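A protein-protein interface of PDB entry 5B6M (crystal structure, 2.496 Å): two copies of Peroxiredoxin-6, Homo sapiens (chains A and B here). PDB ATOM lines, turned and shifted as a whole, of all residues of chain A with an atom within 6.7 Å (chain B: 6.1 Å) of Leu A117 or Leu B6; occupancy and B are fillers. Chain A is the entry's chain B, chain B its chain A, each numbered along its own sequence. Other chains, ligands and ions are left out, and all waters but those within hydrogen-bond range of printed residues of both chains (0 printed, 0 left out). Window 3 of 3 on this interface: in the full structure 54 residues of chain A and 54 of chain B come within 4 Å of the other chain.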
ATOM      1  N   GLY A   4     -29.268  23.407  14.708  1.00  0.00           N
ATOM      2  CA  GLY A   4     -28.978  24.764  15.117  1.00  0.00           C
ATOM      3  C   GLY A   4     -30.189  25.497  15.678  1.00  0.00           C
ATOM      4  O   GLY A   4     -30.232  25.802  16.875  1.00  0.00           O
ATOM      5  N   ALA A 111     -21.224  30.690  15.254  1.00  0.00           N
ATOM      6  CA  ALA A 111     -21.341  29.784  14.107  1.00  0.00           C
ATOM      7  C   ALA A 111     -21.799  28.406  14.555  1.00  0.00           C
ATOM      8  O   ALA A 111     -22.791  27.873  14.045  1.00  0.00           O
ATOM      9  CB  ALA A 111     -20.037  29.705  13.304  1.00  0.00           C
ATOM     10  N   ILE A 112     -21.098  27.843  15.534  1.00  0.00           N
ATOM     11  CA  ILE A 112     -21.470  26.537  16.056  1.00  0.00           C
ATOM     12  C   ILE A 112     -22.815  26.623  16.802  1.00  0.00           C
ATOM     13  O   ILE A 112     -23.662  25.725  16.679  1.00  0.00           O
ATOM     14  CB  ILE A 112     -20.327  25.916  16.906  1.00  0.00           C
ATOM     15  CG1 ILE A 112     -19.353  25.126  16.012  1.00  0.00           C
ATOM     16  CG2 ILE A 112     -20.876  25.000  17.986  1.00  0.00           C
ATOM     17  CD1 ILE A 112     -19.856  23.734  15.596  1.00  0.00           C
ATOM     18  N   LEU A 113     -23.025  27.729  17.522  1.00  0.00           N
ATOM     19  CA  LEU A 113     -24.284  27.995  18.248  1.00  0.00           C
ATOM     20  C   LEU A 113     -25.559  27.908  17.370  1.00  0.00           C
ATOM     21  O   LEU A 113     -26.514  27.189  17.703  1.00  0.00           O
ATOM     22  CB  LEU A 113     -24.221  29.384  18.910  1.00  0.00           C
ATOM     23  CG  LEU A 113     -24.878  29.654  20.277  1.00  0.00           C
ATOM     24  CD1 LEU A 113     -25.616  31.003  20.292  1.00  0.00           C
ATOM     25  CD2 LEU A 113     -25.795  28.520  20.733  1.00  0.00           C
ATOM     26  N   LEU A 114     -25.566  28.653  16.263  1.00  0.00           N
ATOM     27  CA  LEU A 114     -26.740  28.759  15.406  1.00  0.00           C
ATOM     28  C   LEU A 114     -26.671  27.743  14.271  1.00  0.00           C
ATOM     29  O   LEU A 114     -27.597  27.635  13.459  1.00  0.00           O
ATOM     30  CB  LEU A 114     -26.866  30.181  14.865  1.00  0.00           C
ATOM     31  CG  LEU A 114     -26.803  31.208  15.988  1.00  0.00           C
ATOM     32  CD1 LEU A 114     -26.855  32.622  15.478  1.00  0.00           C
ATOM     33  CD2 LEU A 114     -27.945  30.959  16.924  1.00  0.00           C
ATOM     34  N   GLY A 115     -25.573  26.996  14.225  1.00  0.00           N
ATOM     35  CA  GLY A 115     -25.420  25.950  13.239  1.00  0.00           C
ATOM     36  C   GLY A 115     -25.154  26.489  11.847  1.00  0.00           C
ATOM     37  O   GLY A 115     -25.660  25.950  10.861  1.00  0.00           O
ATOM     38  N   MET A 116     -24.338  27.537  11.764  1.00  0.00           N
ATOM     39  CA  MET A 116     -24.019  28.170  10.486  1.00  0.00           C
ATOM     40  C   MET A 116     -22.788  27.592   9.761  1.00  0.00           C
ATOM     41  O   MET A 116     -22.477  27.991   8.651  1.00  0.00           O
ATOM     42  CB  MET A 116     -23.879  29.677  10.695  1.00  0.00           C
ATOM     43  CG  MET A 116     -24.900  30.191  11.672  1.00  0.00           C
ATOM     44  SD  MET A 116     -24.900  31.976  11.834  1.00  0.00           S
ATOM     45  CE  MET A 116     -23.436  32.225  12.835  1.00  0.00           C
ATOM     46  N   LEU A 117     -22.103  26.646  10.384  1.00  0.00           N
ATOM     47  CA  LEU A 117     -20.899  26.029   9.824  1.00  0.00           C
ATOM     48  C   LEU A 117     -21.101  25.475   8.399  1.00  0.00           C
ATOM     49  O   LEU A 117     -22.062  24.764   8.141  1.00  0.00           O
ATOM     50  CB  LEU A 117     -20.476  24.891  10.751  1.00  0.00           C
ATOM     51  CG  LEU A 117     -21.671  23.958  11.053  1.00  0.00           C
ATOM     52  CD1 LEU A 117     -21.401  22.486  10.661  1.00  0.00           C
ATOM     53  CD2 LEU A 117     -22.164  24.082  12.503  1.00  0.00           C
ATOM     54  N   ASP A 118     -20.194  25.793   7.476  1.00  0.00           N
ATOM     55  CA  ASP A 118     -20.288  25.288   6.098  1.00  0.00           C
ATOM     56  C   ASP A 118     -19.522  23.962   5.941  1.00  0.00           C
ATOM     57  O   ASP A 118     -18.516  23.732   6.622  1.00  0.00           O
ATOM     58  CB  ASP A 118     -19.785  26.358   5.114  1.00  0.00           C
ATOM     59  CG  ASP A 118     -19.872  25.925   3.650  1.00  0.00           C
ATOM     60  OD1 ASP A 118     -18.990  25.154   3.214  1.00  0.00           O
ATOM     61  OD2 ASP A 118     -20.792  26.372   2.927  1.00  0.00           O
ATOM     62  N   PRO A 119     -20.007  23.067   5.061  1.00  0.00           N
ATOM     63  CA  PRO A 119     -19.320  21.779   4.921  1.00  0.00           C
ATOM     64  C   PRO A 119     -18.143  21.821   3.948  1.00  0.00           C
ATOM     65  O   PRO A 119     -17.150  21.126   4.164  1.00  0.00           O
ATOM     66  CB  PRO A 119     -20.415  20.864   4.370  1.00  0.00           C
ATOM     67  CG  PRO A 119     -21.269  21.769   3.575  1.00  0.00           C
ATOM     68  CD  PRO A 119     -21.268  23.095   4.302  1.00  0.00           C
ATOM     69  N   GLU A 121     -16.259  24.613   2.834  1.00  0.00           N
ATOM     70  CA  GLU A 121     -15.407  25.806   2.815  1.00  0.00           C
ATOM     71  C   GLU A 121     -14.674  26.096   4.122  1.00  0.00           C
ATOM     72  O   GLU A 121     -15.273  26.101   5.201  1.00  0.00           O
ATOM     73  CB  GLU A 121     -16.195  27.035   2.355  1.00  0.00           C
ATOM     74  CG  GLU A 121     -16.343  27.132   0.849  1.00  0.00           C
ATOM     75  CD  GLU A 121     -15.907  28.479   0.317  1.00  0.00           C
ATOM     76  OE1 GLU A 121     -15.482  29.315   1.146  1.00  0.00           O
ATOM     77  OE2 GLU A 121     -15.988  28.697  -0.918  1.00  0.00           O
ATOM     78  N   PRO A 128     -13.108  25.556   9.520  1.00  0.00           N
ATOM     79  CA  PRO A 128     -14.211  25.763   8.572  1.00  0.00           C
ATOM     80  C   PRO A 128     -14.892  27.107   8.810  1.00  0.00           C
ATOM     81  O   PRO A 128     -14.731  27.696   9.884  1.00  0.00           O
ATOM     82  CB  PRO A 128     -15.186  24.623   8.903  1.00  0.00           C
ATOM     83  CG  PRO A 128     -14.519  23.790   9.985  1.00  0.00           C
ATOM     84  CD  PRO A 128     -13.515  24.685  10.634  1.00  0.00           C
ATOM     85  N   VAL A 129     -15.651  27.584   7.830  1.00  0.00           N
ATOM     86  CA  VAL A 129     -16.287  28.890   7.957  1.00  0.00           C
ATOM     87  C   VAL A 129     -17.808  28.783   7.887  1.00  0.00           C
ATOM     88  O   VAL A 129     -18.353  27.682   7.775  1.00  0.00           O
ATOM     89  CB  VAL A 129     -15.801  29.842   6.872  1.00  0.00           C
ATOM     90  CG1 VAL A 129     -14.288  30.020   6.964  1.00  0.00           C
ATOM     91  CG2 VAL A 129     -16.224  29.317   5.501  1.00  0.00           C
ATOM     92  N   THR A 130     -18.491  29.927   7.962  1.00  0.00           N
ATOM     93  CA  THR A 130     -19.945  29.939   7.908  1.00  0.00           C
ATOM     94  C   THR A 130     -20.409  29.825   6.470  1.00  0.00           C
ATOM     95  O   THR A 130     -19.668  30.135   5.541  1.00  0.00           O
ATOM     96  CB  THR A 130     -20.585  31.224   8.494  1.00  0.00           C
ATOM     97  OG1 THR A 130     -20.173  32.364   7.737  1.00  0.00           O
ATOM     98  CG2 THR A 130     -20.203  31.412   9.931  1.00  0.00           C
ATOM     99  N   ALA A 131     -21.645  29.373   6.304  1.00  0.00           N
ATOM    100  CA  ALA A 131     -22.298  29.354   5.017  1.00  0.00           C
ATOM    101  C   ALA A 131     -23.298  30.494   5.072  1.00  0.00           C
ATOM    102  O   ALA A 131     -23.452  31.139   6.112  1.00  0.00           O
ATOM    103  CB  ALA A 131     -23.225  28.173   4.926  1.00  0.00           C
ATOM    104  N   LEU A 148     -30.830  28.541   4.443  1.00  0.00           N
ATOM    105  CA  LEU A 148     -29.488  27.993   4.583  1.00  0.00           C
ATOM    106  C   LEU A 148     -28.844  27.750   3.216  1.00  0.00           C
ATOM    107  O   LEU A 148     -28.957  26.650   2.643  1.00  0.00           O
ATOM    108  CB  LEU A 148     -29.555  26.668   5.335  1.00  0.00           C
ATOM    109  CG  LEU A 148     -28.452  26.295   6.317  1.00  0.00           C
ATOM    110  CD1 LEU A 148     -28.249  24.777   6.350  1.00  0.00           C
ATOM    111  CD2 LEU A 148     -27.161  27.026   6.023  1.00  0.00           C
ATOM    112  N   GLY B   4     -32.437  20.416  13.834  1.00  0.00           N
ATOM    113  CA  GLY B   4     -32.985  19.517  12.832  1.00  0.00           C
ATOM    114  C   GLY B   4     -31.990  18.969  11.810  1.00  0.00           C
ATOM    115  O   GLY B   4     -31.579  17.809  11.888  1.00  0.00           O
ATOM    116  N   LEU B   5     -31.613  19.784  10.831  1.00  0.00           N
ATOM    117  CA  LEU B   5     -30.651  19.345   9.823  1.00  0.00           C
ATOM    118  C   LEU B   5     -29.694  20.469   9.467  1.00  0.00           C
ATOM    119  O   LEU B   5     -30.077  21.641   9.490  1.00  0.00           O
ATOM    120  CB  LEU B   5     -31.363  18.850   8.561  1.00  0.00           C
ATOM    121  CG  LEU B   5     -30.530  17.947   7.654  1.00  0.00           C
ATOM    122  CD1 LEU B   5     -29.790  16.973   8.511  1.00  0.00           C
ATOM    123  CD2 LEU B   5     -31.415  17.194   6.678  1.00  0.00           C
ATOM    124  N   LEU B   6     -28.448  20.123   9.156  1.00  0.00           N
ATOM    125  CA  LEU B   6     -27.515  21.151   8.697  1.00  0.00           C
ATOM    126  C   LEU B   6     -26.562  20.737   7.545  1.00  0.00           C
ATOM    127  O   LEU B   6     -26.437  19.570   7.207  1.00  0.00           O
ATOM    128  CB  LEU B   6     -26.826  21.875   9.878  1.00  0.00           C
ATOM    129  CG  LEU B   6     -25.954  21.182  10.923  1.00  0.00           C
ATOM    130  CD1 LEU B   6     -24.623  20.763  10.314  1.00  0.00           C
ATOM    131  CD2 LEU B   6     -25.732  22.095  12.129  1.00  0.00           C
ATOM    132  N   LEU B   7     -25.929  21.725   6.932  1.00  0.00           N
ATOM    133  CA  LEU B   7     -25.233  21.558   5.660  1.00  0.00           C
ATOM    134  C   LEU B   7     -24.173  20.455   5.647  1.00  0.00           C
ATOM    135  O   LEU B   7     -23.295  20.402   6.514  1.00  0.00           O
ATOM    136  CB  LEU B   7     -24.631  22.899   5.243  1.00  0.00           C
ATOM    137  CG  LEU B   7     -25.140  23.519   3.946  1.00  0.00           C
ATOM    138  CD1 LEU B   7     -26.602  23.193   3.709  1.00  0.00           C
ATOM    139  CD2 LEU B   7     -24.933  25.027   3.952  1.00  0.00           C
ATOM    140  N   GLY B   8     -24.259  19.573   4.656  1.00  0.00           N
ATOM    141  CA  GLY B   8     -23.336  18.461   4.559  1.00  0.00           C
ATOM    142  C   GLY B   8     -23.846  17.180   5.207  1.00  0.00           C
ATOM    143  O   GLY B   8     -23.301  16.104   4.938  1.00  0.00           O
ATOM    144  N   ASP B   9     -24.875  17.275   6.055  1.00  0.00           N
ATOM    145  CA  ASP B   9     -25.480  16.081   6.655  1.00  0.00           C
ATOM    146  C   ASP B   9     -26.121  15.172   5.593  1.00  0.00           C
ATOM    147  O   ASP B   9     -26.756  15.650   4.640  1.00  0.00           O
ATOM    148  CB  ASP B   9     -26.535  16.434   7.719  1.00  0.00           C
ATOM    149  CG  ASP B   9     -25.955  17.171   8.930  1.00  0.00           C
ATOM    150  OD1 ASP B   9     -24.721  17.122   9.128  1.00  0.00           O
ATOM    151  OD2 ASP B   9     -26.741  17.803   9.682  1.00  0.00           O
ATOM    152  N   VAL B  10     -25.947  13.863   5.764  1.00  0.00           N
ATOM    153  CA  VAL B  10     -26.550  12.875   4.878  1.00  0.00           C
ATOM    154  C   VAL B  10     -28.058  12.734   5.164  1.00  0.00           C
ATOM    155  O   VAL B  10     -28.497  12.818   6.319  1.00  0.00           O
ATOM    156  CB  VAL B  10     -25.808  11.515   4.996  1.00  0.00           C
ATOM    157  CG1 VAL B  10     -26.484  10.423   4.177  1.00  0.00           C
ATOM    158  CG2 VAL B  10     -24.365  11.685   4.556  1.00  0.00           C
ATOM    159  N   LEU B 143     -27.027  17.091   2.463  1.00  0.00           N
ATOM    160  CA  LEU B 143     -27.807  18.311   2.377  1.00  0.00           C
ATOM    161  C   LEU B 143     -26.989  19.408   1.695  1.00  0.00           C
ATOM    162  O   LEU B 143     -25.878  19.716   2.121  1.00  0.00           O
ATOM    163  CB  LEU B 143     -28.265  18.771   3.763  1.00  0.00           C
ATOM    164  CG  LEU B 143     -29.063  20.075   3.738  1.00  0.00           C
ATOM    165  CD1 LEU B 143     -30.285  19.923   2.833  1.00  0.00           C
ATOM    166  CD2 LEU B 143     -29.469  20.567   5.129  1.00  0.00           C
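N of Leu B6 lies within hydrogen-bond range of OD2 of Asp B9.
The backbone NH (N) of Gly B8 lies within hydrogen-bond range of the backbone carbonyl oxygen (O) of Leu B143 (3.0 Å).
The backbone carbonyl oxygen (O) of Met A116 lies within hydrogen-bond range of the backbone NH (N) of Ala A131.
Among the printed residues, merely in contact across the chains: Leu A117 with Leu B6 (3.7 Å), Pro A119 with Leu B7 (3.5 Å), Pro A119 with Gly B8 (3.8 Å), Ala A131 with Leu B7 (3.7 Å) and Leu A148 with Leu B7 (3.5 Å).
Of chain B, only Leu B6 comes within 4 Å of Leu A117.
Leu B6 touches just one residue of chain A: Leu A117.
Printed residues of chain A within 4 Å of Gly B8: Pro A119 (3.8 Å).
Printed residues of chain A within 4 Å of Leu B7: Pro A119 (3.5 Å), Ala A131 (3.7 Å) and Leu A148 (3.5 Å).
Printed residues of chain B within 4 Å of Pro A119: Leu B7 (3.5 Å) and Gly B8 (3.8 Å).
Of the printed residues of chain B, Ala A131 touches Leu B7 (3.7 Å).
Leu B143 touches none of the printed residues of chain A.
Asp A118 touches none of the printed residues of chain B.
The nearest printed residue of chain B that does not touch Leu A148 is Leu B6 (4.4 Å).
Hydrophobic or aromatic side chains of chain B within 4 Å of the printed part of chain A: Leu B6 and Leu B7.
Of the 16 printed residues of chain A, 4 touch a printed residue of chain B.
Printed residues of chain A that touch a printed residue of chain B: Leu A117, Pro A119, Ala A131 and Leu A148.
Among the printed residues, 5 pairs touch across the chains.
Among the printed residues, no Asp or Glu carboxylate lies within 4 Å of a Lys or Arg side-chain nitrogen of the other chain.
Position printed for both chains: 4.
Of the 5 pairs that touch across the chains among the printed residues, none has its exchanged pair printed and touching as well.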
